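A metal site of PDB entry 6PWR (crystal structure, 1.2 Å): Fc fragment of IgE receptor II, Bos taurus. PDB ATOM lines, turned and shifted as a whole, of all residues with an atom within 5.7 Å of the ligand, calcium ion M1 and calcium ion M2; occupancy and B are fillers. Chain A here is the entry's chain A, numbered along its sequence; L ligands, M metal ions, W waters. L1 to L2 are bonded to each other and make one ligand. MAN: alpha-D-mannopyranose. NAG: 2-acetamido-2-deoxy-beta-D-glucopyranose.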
ATOM      1  N   ARG A  63     -20.378  25.976  14.822  1.00  0.00           N
ATOM      2  CA  ARG A  63     -19.079  25.359  14.630  1.00  0.00           C
ATOM      3  C   ARG A  63     -18.502  25.598  13.240  1.00  0.00           C
ATOM      4  O   ARG A  63     -17.441  25.059  12.921  1.00  0.00           O
ATOM      5  CB  ARG A  63     -19.142  23.872  14.959  1.00  0.00           C
ATOM      6  CG  ARG A  63     -19.360  23.625  16.462  1.00  0.00           C
ATOM      7  CD  ARG A  63     -19.261  22.160  16.823  1.00  0.00           C
ATOM      8  NE  ARG A  63     -20.319  21.373  16.195  1.00  0.00           N
ATOM      9  CZ  ARG A  63     -20.317  20.050  16.146  1.00  0.00           C
ATOM     10  NH1 ARG A  63     -19.302  19.370  16.673  1.00  0.00           N
ATOM     11  NH2 ARG A  63     -21.306  19.400  15.568  1.00  0.00           N
ATOM     12  N   ASP A  71     -11.006  29.692  -4.087  1.00  0.00           N
ATOM     13  CA  ASP A  71      -9.978  30.160  -5.018  1.00  0.00           C
ATOM     14  C   ASP A  71      -9.114  28.990  -5.472  1.00  0.00           C
ATOM     15  O   ASP A  71      -7.914  29.134  -5.694  1.00  0.00           O
ATOM     16  CB  ASP A  71      -9.172  31.349  -4.465  1.00  0.00           C
ATOM     17  CG  ASP A  71      -8.221  30.982  -3.325  1.00  0.00           C
ATOM     18  OD1 ASP A  71      -8.435  29.979  -2.615  1.00  0.00           O
ATOM     19  OD2 ASP A  71      -7.216  31.706  -3.117  1.00  0.00           O
ATOM     20  N   GLU A  75      -5.197  31.123  -7.322  1.00  0.00           N
ATOM     21  CA  GLU A  75      -5.054  31.632  -5.965  1.00  0.00           C
ATOM     22  C   GLU A  75      -5.424  33.118  -5.928  1.00  0.00           C
ATOM     23  O   GLU A  75      -4.997  33.904  -6.784  1.00  0.00           O
ATOM     24  CB  GLU A  75      -3.623  31.450  -5.491  1.00  0.00           C
ATOM     25  CG  GLU A  75      -3.349  32.021  -4.109  1.00  0.00           C
ATOM     26  CD  GLU A  75      -4.198  31.364  -3.022  1.00  0.00           C
ATOM     27  OE1 GLU A  75      -4.597  30.188  -3.194  1.00  0.00           O
ATOM     28  OE2 GLU A  75      -4.462  32.032  -2.008  1.00  0.00           O
ATOM     29  N   GLY A  76      -6.218  33.486  -4.937  1.00  0.00           N
ATOM     30  CA  GLY A  76      -6.643  34.845  -4.750  1.00  0.00           C
ATOM     31  C   GLY A  76      -7.744  35.298  -5.663  1.00  0.00           C
ATOM     32  O   GLY A  76      -8.217  36.432  -5.532  1.00  0.00           O
ATOM     33  N   PHE A  78     -11.318  34.472  -6.168  1.00  0.00           N
ATOM     34  CA  PHE A  78     -12.410  33.689  -5.629  1.00  0.00           C
ATOM     35  C   PHE A  78     -13.549  33.635  -6.621  1.00  0.00           C
ATOM     36  O   PHE A  78     -13.810  34.590  -7.353  1.00  0.00           O
ATOM     37  CB  PHE A  78     -12.861  34.240  -4.273  1.00  0.00           C
ATOM     38  CG  PHE A  78     -11.894  33.926  -3.185  1.00  0.00           C
ATOM     39  CD1 PHE A  78     -10.830  34.768  -2.924  1.00  0.00           C
ATOM     40  CD2 PHE A  78     -11.991  32.742  -2.491  1.00  0.00           C
ATOM     41  CE1 PHE A  78      -9.915  34.453  -1.951  1.00  0.00           C
ATOM     42  CE2 PHE A  78     -11.074  32.419  -1.525  1.00  0.00           C
ATOM     43  CZ  PHE A  78     -10.030  33.281  -1.260  1.00  0.00           C
ATOM     44  N   GLU A  95      -8.744  37.789   6.985  1.00  0.00           N
ATOM     45  CA  GLU A  95      -9.036  36.744   6.039  1.00  0.00           C
ATOM     46  C   GLU A  95      -9.421  37.352   4.698  1.00  0.00           C
ATOM     47  O   GLU A  95      -9.878  38.503   4.639  1.00  0.00           O
ATOM     48  CB  GLU A  95     -10.212  35.887   6.532  1.00  0.00           C
ATOM     49  CG  GLU A  95     -10.027  35.326   7.922  1.00  0.00           C
ATOM     50  CD  GLU A  95      -8.838  34.399   8.073  1.00  0.00           C
ATOM     51  OE1 GLU A  95      -8.325  33.872   7.062  1.00  0.00           O
ATOM     52  OE2 GLU A  95      -8.424  34.204   9.238  1.00  0.00           O
ATOM     53  N   PRO A  96      -9.242  36.637   3.594  1.00  0.00           N
ATOM     54  CA  PRO A  96      -8.582  35.334   3.539  1.00  0.00           C
ATOM     55  C   PRO A  96      -7.080  35.508   3.700  1.00  0.00           C
ATOM     56  O   PRO A  96      -6.514  36.513   3.239  1.00  0.00           O
ATOM     57  CB  PRO A  96      -8.919  34.845   2.129  1.00  0.00           C
ATOM     58  CG  PRO A  96      -9.067  36.106   1.337  1.00  0.00           C
ATOM     59  CD  PRO A  96      -9.655  37.118   2.262  1.00  0.00           C
ATOM     60  N   ASN A  97      -6.460  34.571   4.385  1.00  0.00           N
ATOM     61  CA  ASN A  97      -5.036  34.652   4.654  1.00  0.00           C
ATOM     62  C   ASN A  97      -4.213  33.526   4.056  1.00  0.00           C
ATOM     63  O   ASN A  97      -2.988  33.522   4.217  1.00  0.00           O
ATOM     64  CB  ASN A  97      -4.751  34.790   6.157  1.00  0.00           C
ATOM     65  CG  ASN A  97      -5.184  33.582   6.954  1.00  0.00           C
ATOM     66  OD1 ASN A  97      -5.717  32.615   6.412  1.00  0.00           O
ATOM     67  ND2 ASN A  97      -4.942  33.623   8.254  1.00  0.00           N
ATOM     68  N   ASP A  98      -4.850  32.594   3.347  1.00  0.00           N
ATOM     69  CA  ASP A  98      -4.175  31.473   2.691  1.00  0.00           C
ATOM     70  C   ASP A  98      -3.152  30.804   3.621  1.00  0.00           C
ATOM     71  O   ASP A  98      -1.991  30.597   3.259  1.00  0.00           O
ATOM     72  CB  ASP A  98      -3.538  31.887   1.367  1.00  0.00           C
ATOM     73  CG  ASP A  98      -3.368  30.712   0.422  1.00  0.00           C
ATOM     74  OD1 ASP A  98      -4.334  29.950   0.248  1.00  0.00           O
ATOM     75  OD2 ASP A  98      -2.264  30.551  -0.137  1.00  0.00           O
ATOM     76  N   ALA A  99      -3.603  30.490   4.828  1.00  0.00           N
ATOM     77  CA  ALA A  99      -2.714  30.047   5.885  1.00  0.00           C
ATOM     78  C   ALA A  99      -2.204  28.633   5.630  1.00  0.00           C
ATOM     79  O   ALA A  99      -2.707  27.892   4.783  1.00  0.00           O
ATOM     80  CB  ALA A  99      -3.416  30.109   7.237  1.00  0.00           C
ATOM     81  N   GLY A 102      -1.984  26.365   2.415  1.00  0.00           N
ATOM     82  CA  GLY A 102      -2.870  26.919   1.418  1.00  0.00           C
ATOM     83  C   GLY A 102      -4.306  26.640   1.813  1.00  0.00           C
ATOM     84  O   GLY A 102      -4.662  25.519   2.170  1.00  0.00           O
ATOM     85  N   GLU A 103      -5.126  27.675   1.771  1.00  0.00           N
ATOM     86  CA  GLU A 103      -6.529  27.589   2.147  1.00  0.00           C
ATOM     87  C   GLU A 103      -7.321  28.107   0.962  1.00  0.00           C
ATOM     88  O   GLU A 103      -7.242  29.294   0.629  1.00  0.00           O
ATOM     89  CB  GLU A 103      -6.790  28.408   3.401  1.00  0.00           C
ATOM     90  CG  GLU A 103      -6.043  27.864   4.602  1.00  0.00           C
ATOM     91  CD  GLU A 103      -6.371  28.597   5.871  1.00  0.00           C
ATOM     92  OE1 GLU A 103      -6.426  29.834   5.836  1.00  0.00           O
ATOM     93  OE2 GLU A 103      -6.594  27.937   6.909  1.00  0.00           O
ATOM     94  N   ASN A 104      -8.063  27.220   0.327  1.00  0.00           N
ATOM     95  CA  ASN A 104      -8.684  27.569  -0.933  1.00  0.00           C
ATOM     96  C   ASN A 104     -10.188  27.439  -0.948  1.00  0.00           C
ATOM     97  O   ASN A 104     -10.804  27.659  -1.997  1.00  0.00           O
ATOM     98  CB  ASN A 104      -8.041  26.773  -2.071  1.00  0.00           C
ATOM     99  CG  ASN A 104      -6.542  26.924  -2.093  1.00  0.00           C
ATOM    100  OD1 ASN A 104      -6.010  28.005  -1.834  1.00  0.00           O
ATOM    101  ND2 ASN A 104      -5.849  25.836  -2.367  1.00  0.00           N
ATOM    102  N   MET A 107     -15.351  29.100   4.330  1.00  0.00           N
ATOM    103  CA  MET A 107     -16.373  28.759   5.306  1.00  0.00           C
ATOM    104  C   MET A 107     -16.890  30.033   5.957  1.00  0.00           C
ATOM    105  O   MET A 107     -16.236  31.084   5.970  1.00  0.00           O
ATOM    106  CB  MET A 107     -15.784  27.879   6.425  1.00  0.00           C
ATOM    107  CG  MET A 107     -14.701  28.596   7.206  1.00  0.00           C
ATOM    108  SD  MET A 107     -13.913  27.624   8.486  1.00  0.00           S
ATOM    109  CE  MET A 107     -15.254  27.403   9.623  1.00  0.00           C
ATOM    110  N   LEU A 109     -17.515  31.206   9.681  1.00  0.00           N
ATOM    111  CA  LEU A 109     -17.322  30.916  11.081  1.00  0.00           C
ATOM    112  C   LEU A 109     -18.680  30.899  11.778  1.00  0.00           C
ATOM    113  O   LEU A 109     -19.710  31.220  11.184  1.00  0.00           O
ATOM    114  CB  LEU A 109     -16.444  31.994  11.711  1.00  0.00           C
ATOM    115  CG  LEU A 109     -15.068  32.118  11.067  1.00  0.00           C
ATOM    116  CD1 LEU A 109     -14.319  33.304  11.669  1.00  0.00           C
ATOM    117  CD2 LEU A 109     -14.247  30.847  11.225  1.00  0.00           C
ATOM    118  N   ASN A 115     -13.983  32.813   6.418  1.00  0.00           N
ATOM    119  CA  ASN A 115     -12.591  32.455   6.580  1.00  0.00           C
ATOM    120  C   ASN A 115     -12.242  31.492   5.456  1.00  0.00           C
ATOM    121  O   ASN A 115     -13.018  30.576   5.169  1.00  0.00           O
ATOM    122  CB  ASN A 115     -12.412  31.739   7.910  1.00  0.00           C
ATOM    123  CG  ASN A 115     -11.037  31.151   8.062  1.00  0.00           C
ATOM    124  OD1 ASN A 115     -10.046  31.822   7.793  1.00  0.00           O
ATOM    125  ND2 ASN A 115     -10.963  29.880   8.477  1.00  0.00           N
ATOM    126  N   ASP A 116     -11.091  31.674   4.828  1.00  0.00           N
ATOM    127  CA  ASP A 116     -10.587  30.620   3.972  1.00  0.00           C
ATOM    128  C   ASP A 116      -9.981  29.513   4.817  1.00  0.00           C
ATOM    129  O   ASP A 116      -9.291  29.760   5.805  1.00  0.00           O
ATOM    130  CB  ASP A 116      -9.591  31.126   2.919  1.00  0.00           C
ATOM    131  CG  ASP A 116      -8.366  31.824   3.505  1.00  0.00           C
ATOM    132  OD1 ASP A 116      -8.390  32.263   4.673  1.00  0.00           O
ATOM    133  OD2 ASP A 116      -7.392  31.949   2.732  1.00  0.00           O
ATOM    134  N   ALA A 117     -10.265  28.276   4.429  1.00  0.00           N
ATOM    135  CA  ALA A 117      -9.803  27.127   5.182  1.00  0.00           C
ATOM    136  C   ALA A 117      -9.247  26.098   4.222  1.00  0.00           C
ATOM    137  O   ALA A 117      -9.517  26.115   3.017  1.00  0.00           O
ATOM    138  CB  ALA A 117     -10.933  26.507   6.010  1.00  0.00           C
ATOM    139  N   PHE A 118      -8.484  25.170   4.786  1.00  0.00           N
ATOM    140  CA  PHE A 118      -8.034  24.016   4.036  1.00  0.00           C
ATOM    141  C   PHE A 118      -9.251  23.256   3.517  1.00  0.00           C
ATOM    142  O   PHE A 118     -10.158  22.913   4.273  1.00  0.00           O
ATOM    143  CB  PHE A 118      -7.205  23.125   4.946  1.00  0.00           C
ATOM    144  CG  PHE A 118      -6.862  21.791   4.358  1.00  0.00           C
ATOM    145  CD1 PHE A 118      -6.373  21.680   3.079  1.00  0.00           C
ATOM    146  CD2 PHE A 118      -7.033  20.637   5.105  1.00  0.00           C
ATOM    147  CE1 PHE A 118      -6.045  20.433   2.543  1.00  0.00           C
ATOM    148  CE2 PHE A 118      -6.721  19.401   4.584  1.00  0.00           C
ATOM    149  CZ  PHE A 118      -6.236  19.306   3.301  1.00  0.00           C
ATOM    150  N   SER A 121     -10.430  20.222   5.420  1.00  0.00           N
ATOM    151  CA  SER A 121     -10.963  20.249   6.778  1.00  0.00           C
ATOM    152  C   SER A 121     -12.391  19.718   6.762  1.00  0.00           C
ATOM    153  O   SER A 121     -13.104  19.827   5.761  1.00  0.00           O
ATOM    154  CB  SER A 121     -10.985  21.670   7.323  1.00  0.00           C
ATOM    155  OG  SER A 121      -9.678  22.112   7.595  1.00  0.00           O
ATOM    156  N   LEU A 123     -16.004  20.140   8.308  1.00  0.00           N
ATOM    157  CA  LEU A 123     -16.897  21.021   9.029  1.00  0.00           C
ATOM    158  C   LEU A 123     -18.243  20.337   9.165  1.00  0.00           C
ATOM    159  O   LEU A 123     -18.654  19.577   8.301  1.00  0.00           O
ATOM    160  CB  LEU A 123     -17.097  22.350   8.301  1.00  0.00           C
ATOM    161  CG  LEU A 123     -15.821  23.171   8.120  1.00  0.00           C
ATOM    162  CD1 LEU A 123     -16.134  24.458   7.408  1.00  0.00           C
ATOM    163  CD2 LEU A 123     -15.177  23.443   9.468  1.00  0.00           C
HETATM  164  C1  MAN L   1      -7.079  29.004  12.046  1.00  0.00           C
HETATM  165  C2  MAN L   1      -7.743  28.695  10.689  1.00  0.00           C
HETATM  166  C3  MAN L   1      -7.278  29.706   9.650  1.00  0.00           C
HETATM  167  C4  MAN L   1      -7.542  31.103  10.132  1.00  0.00           C
HETATM  168  C5  MAN L   1      -6.788  31.339  11.442  1.00  0.00           C
HETATM  169  C6  MAN L   1      -7.046  32.715  12.020  1.00  0.00           C
HETATM  170  O1  MAN L   1      -5.736  28.659  11.904  1.00  0.00           O
HETATM  171  O2  MAN L   1      -9.124  28.931  10.790  1.00  0.00           O
HETATM  172  O3  MAN L   1      -7.940  29.539   8.409  1.00  0.00           O
HETATM  173  O4  MAN L   1      -7.121  32.024   9.147  1.00  0.00           O
HETATM  174  O5  MAN L   1      -7.247  30.363  12.415  1.00  0.00           O
HETATM  175  O6  MAN L   1      -6.257  32.865  13.207  1.00  0.00           O
HETATM  176  C1  NAG L   2      -9.828  27.806  11.300  1.00  0.00           C
HETATM  177  C2  NAG L   2     -11.113  28.322  11.939  1.00  0.00           C
HETATM  178  C3  NAG L   2     -11.936  27.151  12.454  1.00  0.00           C
HETATM  179  C4  NAG L   2     -12.136  26.111  11.348  1.00  0.00           C
HETATM  180  C5  NAG L   2     -10.816  25.750  10.686  1.00  0.00           C
HETATM  181  C6  NAG L   2     -10.999  24.873   9.471  1.00  0.00           C
HETATM  182  C7  NAG L   2     -10.758  30.596  12.815  1.00  0.00           C
HETATM  183  C8  NAG L   2     -10.446  31.419  14.029  1.00  0.00           C
HETATM  184  N2  NAG L   2     -10.824  29.266  13.006  1.00  0.00           N
HETATM  185  O3  NAG L   2     -13.200  27.633  12.884  1.00  0.00           O
HETATM  186  O4  NAG L   2     -12.704  24.940  11.911  1.00  0.00           O
HETATM  187  O5  NAG L   2     -10.142  26.936  10.237  1.00  0.00           O
HETATM  188  O6  NAG L   2      -9.757  24.390   8.978  1.00  0.00           O
HETATM  189  O7  NAG L   2     -10.963  31.101  11.716  1.00  0.00           O
HETATM  190 CA    CA M   1      -7.843  31.471   6.824  1.00  0.00          CA
HETATM  191 CA    CA M   2      -6.209  30.357  -1.310  1.00  0.00          CA
HETATM  192  O   HOH W   1     -14.341  25.874  14.764  1.00  0.00           O
HETATM  193  O   HOH W   2      -7.699  25.482   7.572  1.00  0.00           O
HETATM  194  O   HOH W   3     -13.706  29.771  14.720  1.00  0.00           O
HETATM  195  O   HOH W   4      -6.336  30.942  15.392  1.00  0.00           O
HETATM  196  O   HOH W   5     -10.777  28.149  15.538  1.00  0.00           O
HETATM  197  O   HOH W   6      -3.486  28.847  10.569  1.00  0.00           O
HETATM  198  O   HOH W   7     -10.532  33.693  11.080  1.00  0.00           O
HETATM  199  O   HOH W   8      -4.440  27.810  14.035  1.00  0.00           O
HETATM  200  O   HOH W   9      -6.229  36.176  13.055  1.00  0.00           O
HETATM  201  O   HOH W  10      -6.910  32.145   0.065  1.00  0.00           O
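O6 of NAG L2 sits at hydrogen-bond distance from OG of Ser 121.
The side-chain carboxylate (OD2) of Asp 116 sits at hydrogen-bond distance from the backbone NH (N) of Asp 98 (2.7 Å). The side-chain carboxylate (OE1) of Glu 103 lies close to the backbone NH (N) of Ala 99, at 3.1 Å. The backbone carbonyl oxygen (O) of Ala 117 lies within hydrogen-bond range of the backbone NH (N) of Asn 104 (3.3 Å). The backbone carbonyl oxygen (O) of Met 107 sits at hydrogen-bond distance from the backbone NH (N) of Asn 115, at 2.9 Å. OD1 of Asn 97 sits close to N of Ala 99, 3.4 Å away. OD2 of Asp 71 lies close to N of Gly 76 (2.7 Å). The side-chain hydroxyl (OG) of Ser 121 sits close to the backbone carbonyl oxygen (O) of Phe 118, at 3.5 Å.
Met 107 touches the ligand. CD2 of Leu 109 touches O7 of NAG L2 (3.3 Å). Ala 117 touches the ligand. CD2 of Leu 123 touches O4 of NAG L2, 3.8 Å away. Ten residues have an atom within 4 Å of the ligand: Glu 95, Asn 97, Glu 103, Met 107, Leu 109, Asn 115, Asp 116, Ala 117, Ser 121 and Leu 123. The nearest printed residue that does not touch the ligand is Phe 118 (4.4 Å).
Within 4 Å of calcium ion M2: Asp 71, Glu 75, Asp 98, Glu 103 and Asn 104. The nearest printed residue that does not touch calcium ion M2 is Asp 116 (4.5 Å).
The side-chain carboxylate (OD1) of Asp 116 is bound to calcium ion M1 (2.4 Å). Calcium ion M1 is bound by OE1 of Glu 103, 2.4 Å away. The side-chain amide oxygen (OD1) of Asn 115 binds calcium ion M1. The side-chain amide oxygen (OD1) of Asn 97 is bound to calcium ion M1, 2.4 Å away. OE1 of Glu 95 is bound to calcium ion M1 (2.5 Å). O of Asp 116 binds calcium ion M1 (2.5 Å). An oxygen (O4) of MAN L1 is bound to calcium ion M1 (2.5 Å). Calcium ion M1 is bound by O3 of MAN L1, at 2.5 Å. Calcium ion M1 has eight donor atoms within binding distance.
Water W10 is bound to calcium ion M2, 2.4 Å away. Calcium ion M2 is bound by OD1 of Asn 104 (2.4 Å). The backbone carbonyl oxygen (O) of Glu 103 binds calcium ion M2 (2.4 Å). Calcium ion M2 is bound by the side-chain carboxylate (OD2) of Asp 71 (2.5 Å). Calcium ion M2 is bound by OD1 of Asp 98. OE1 of Glu 75 binds calcium ion M2 (2.5 Å). Calcium ion M2 is bound by OE2 of Glu 75 (2.5 Å). OD1 of Asp 71 is bound to calcium ion M2 (2.6 Å). Calcium ion M2 has eight donor atoms within binding distance.
Water W7 bridges an oxygen (O7) of NAG L2 (2.7 Å) and the side-chain carboxylate of Glu 95 (2.8 Å). Water W2 lies within hydrogen-bond range of an oxygen (O6) of NAG L2 (2.7 Å), the side-chain carboxylate (OE2) of Glu 103 (2.8 Å) and the backbone NH (N) of Phe 118 (2.9 Å).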
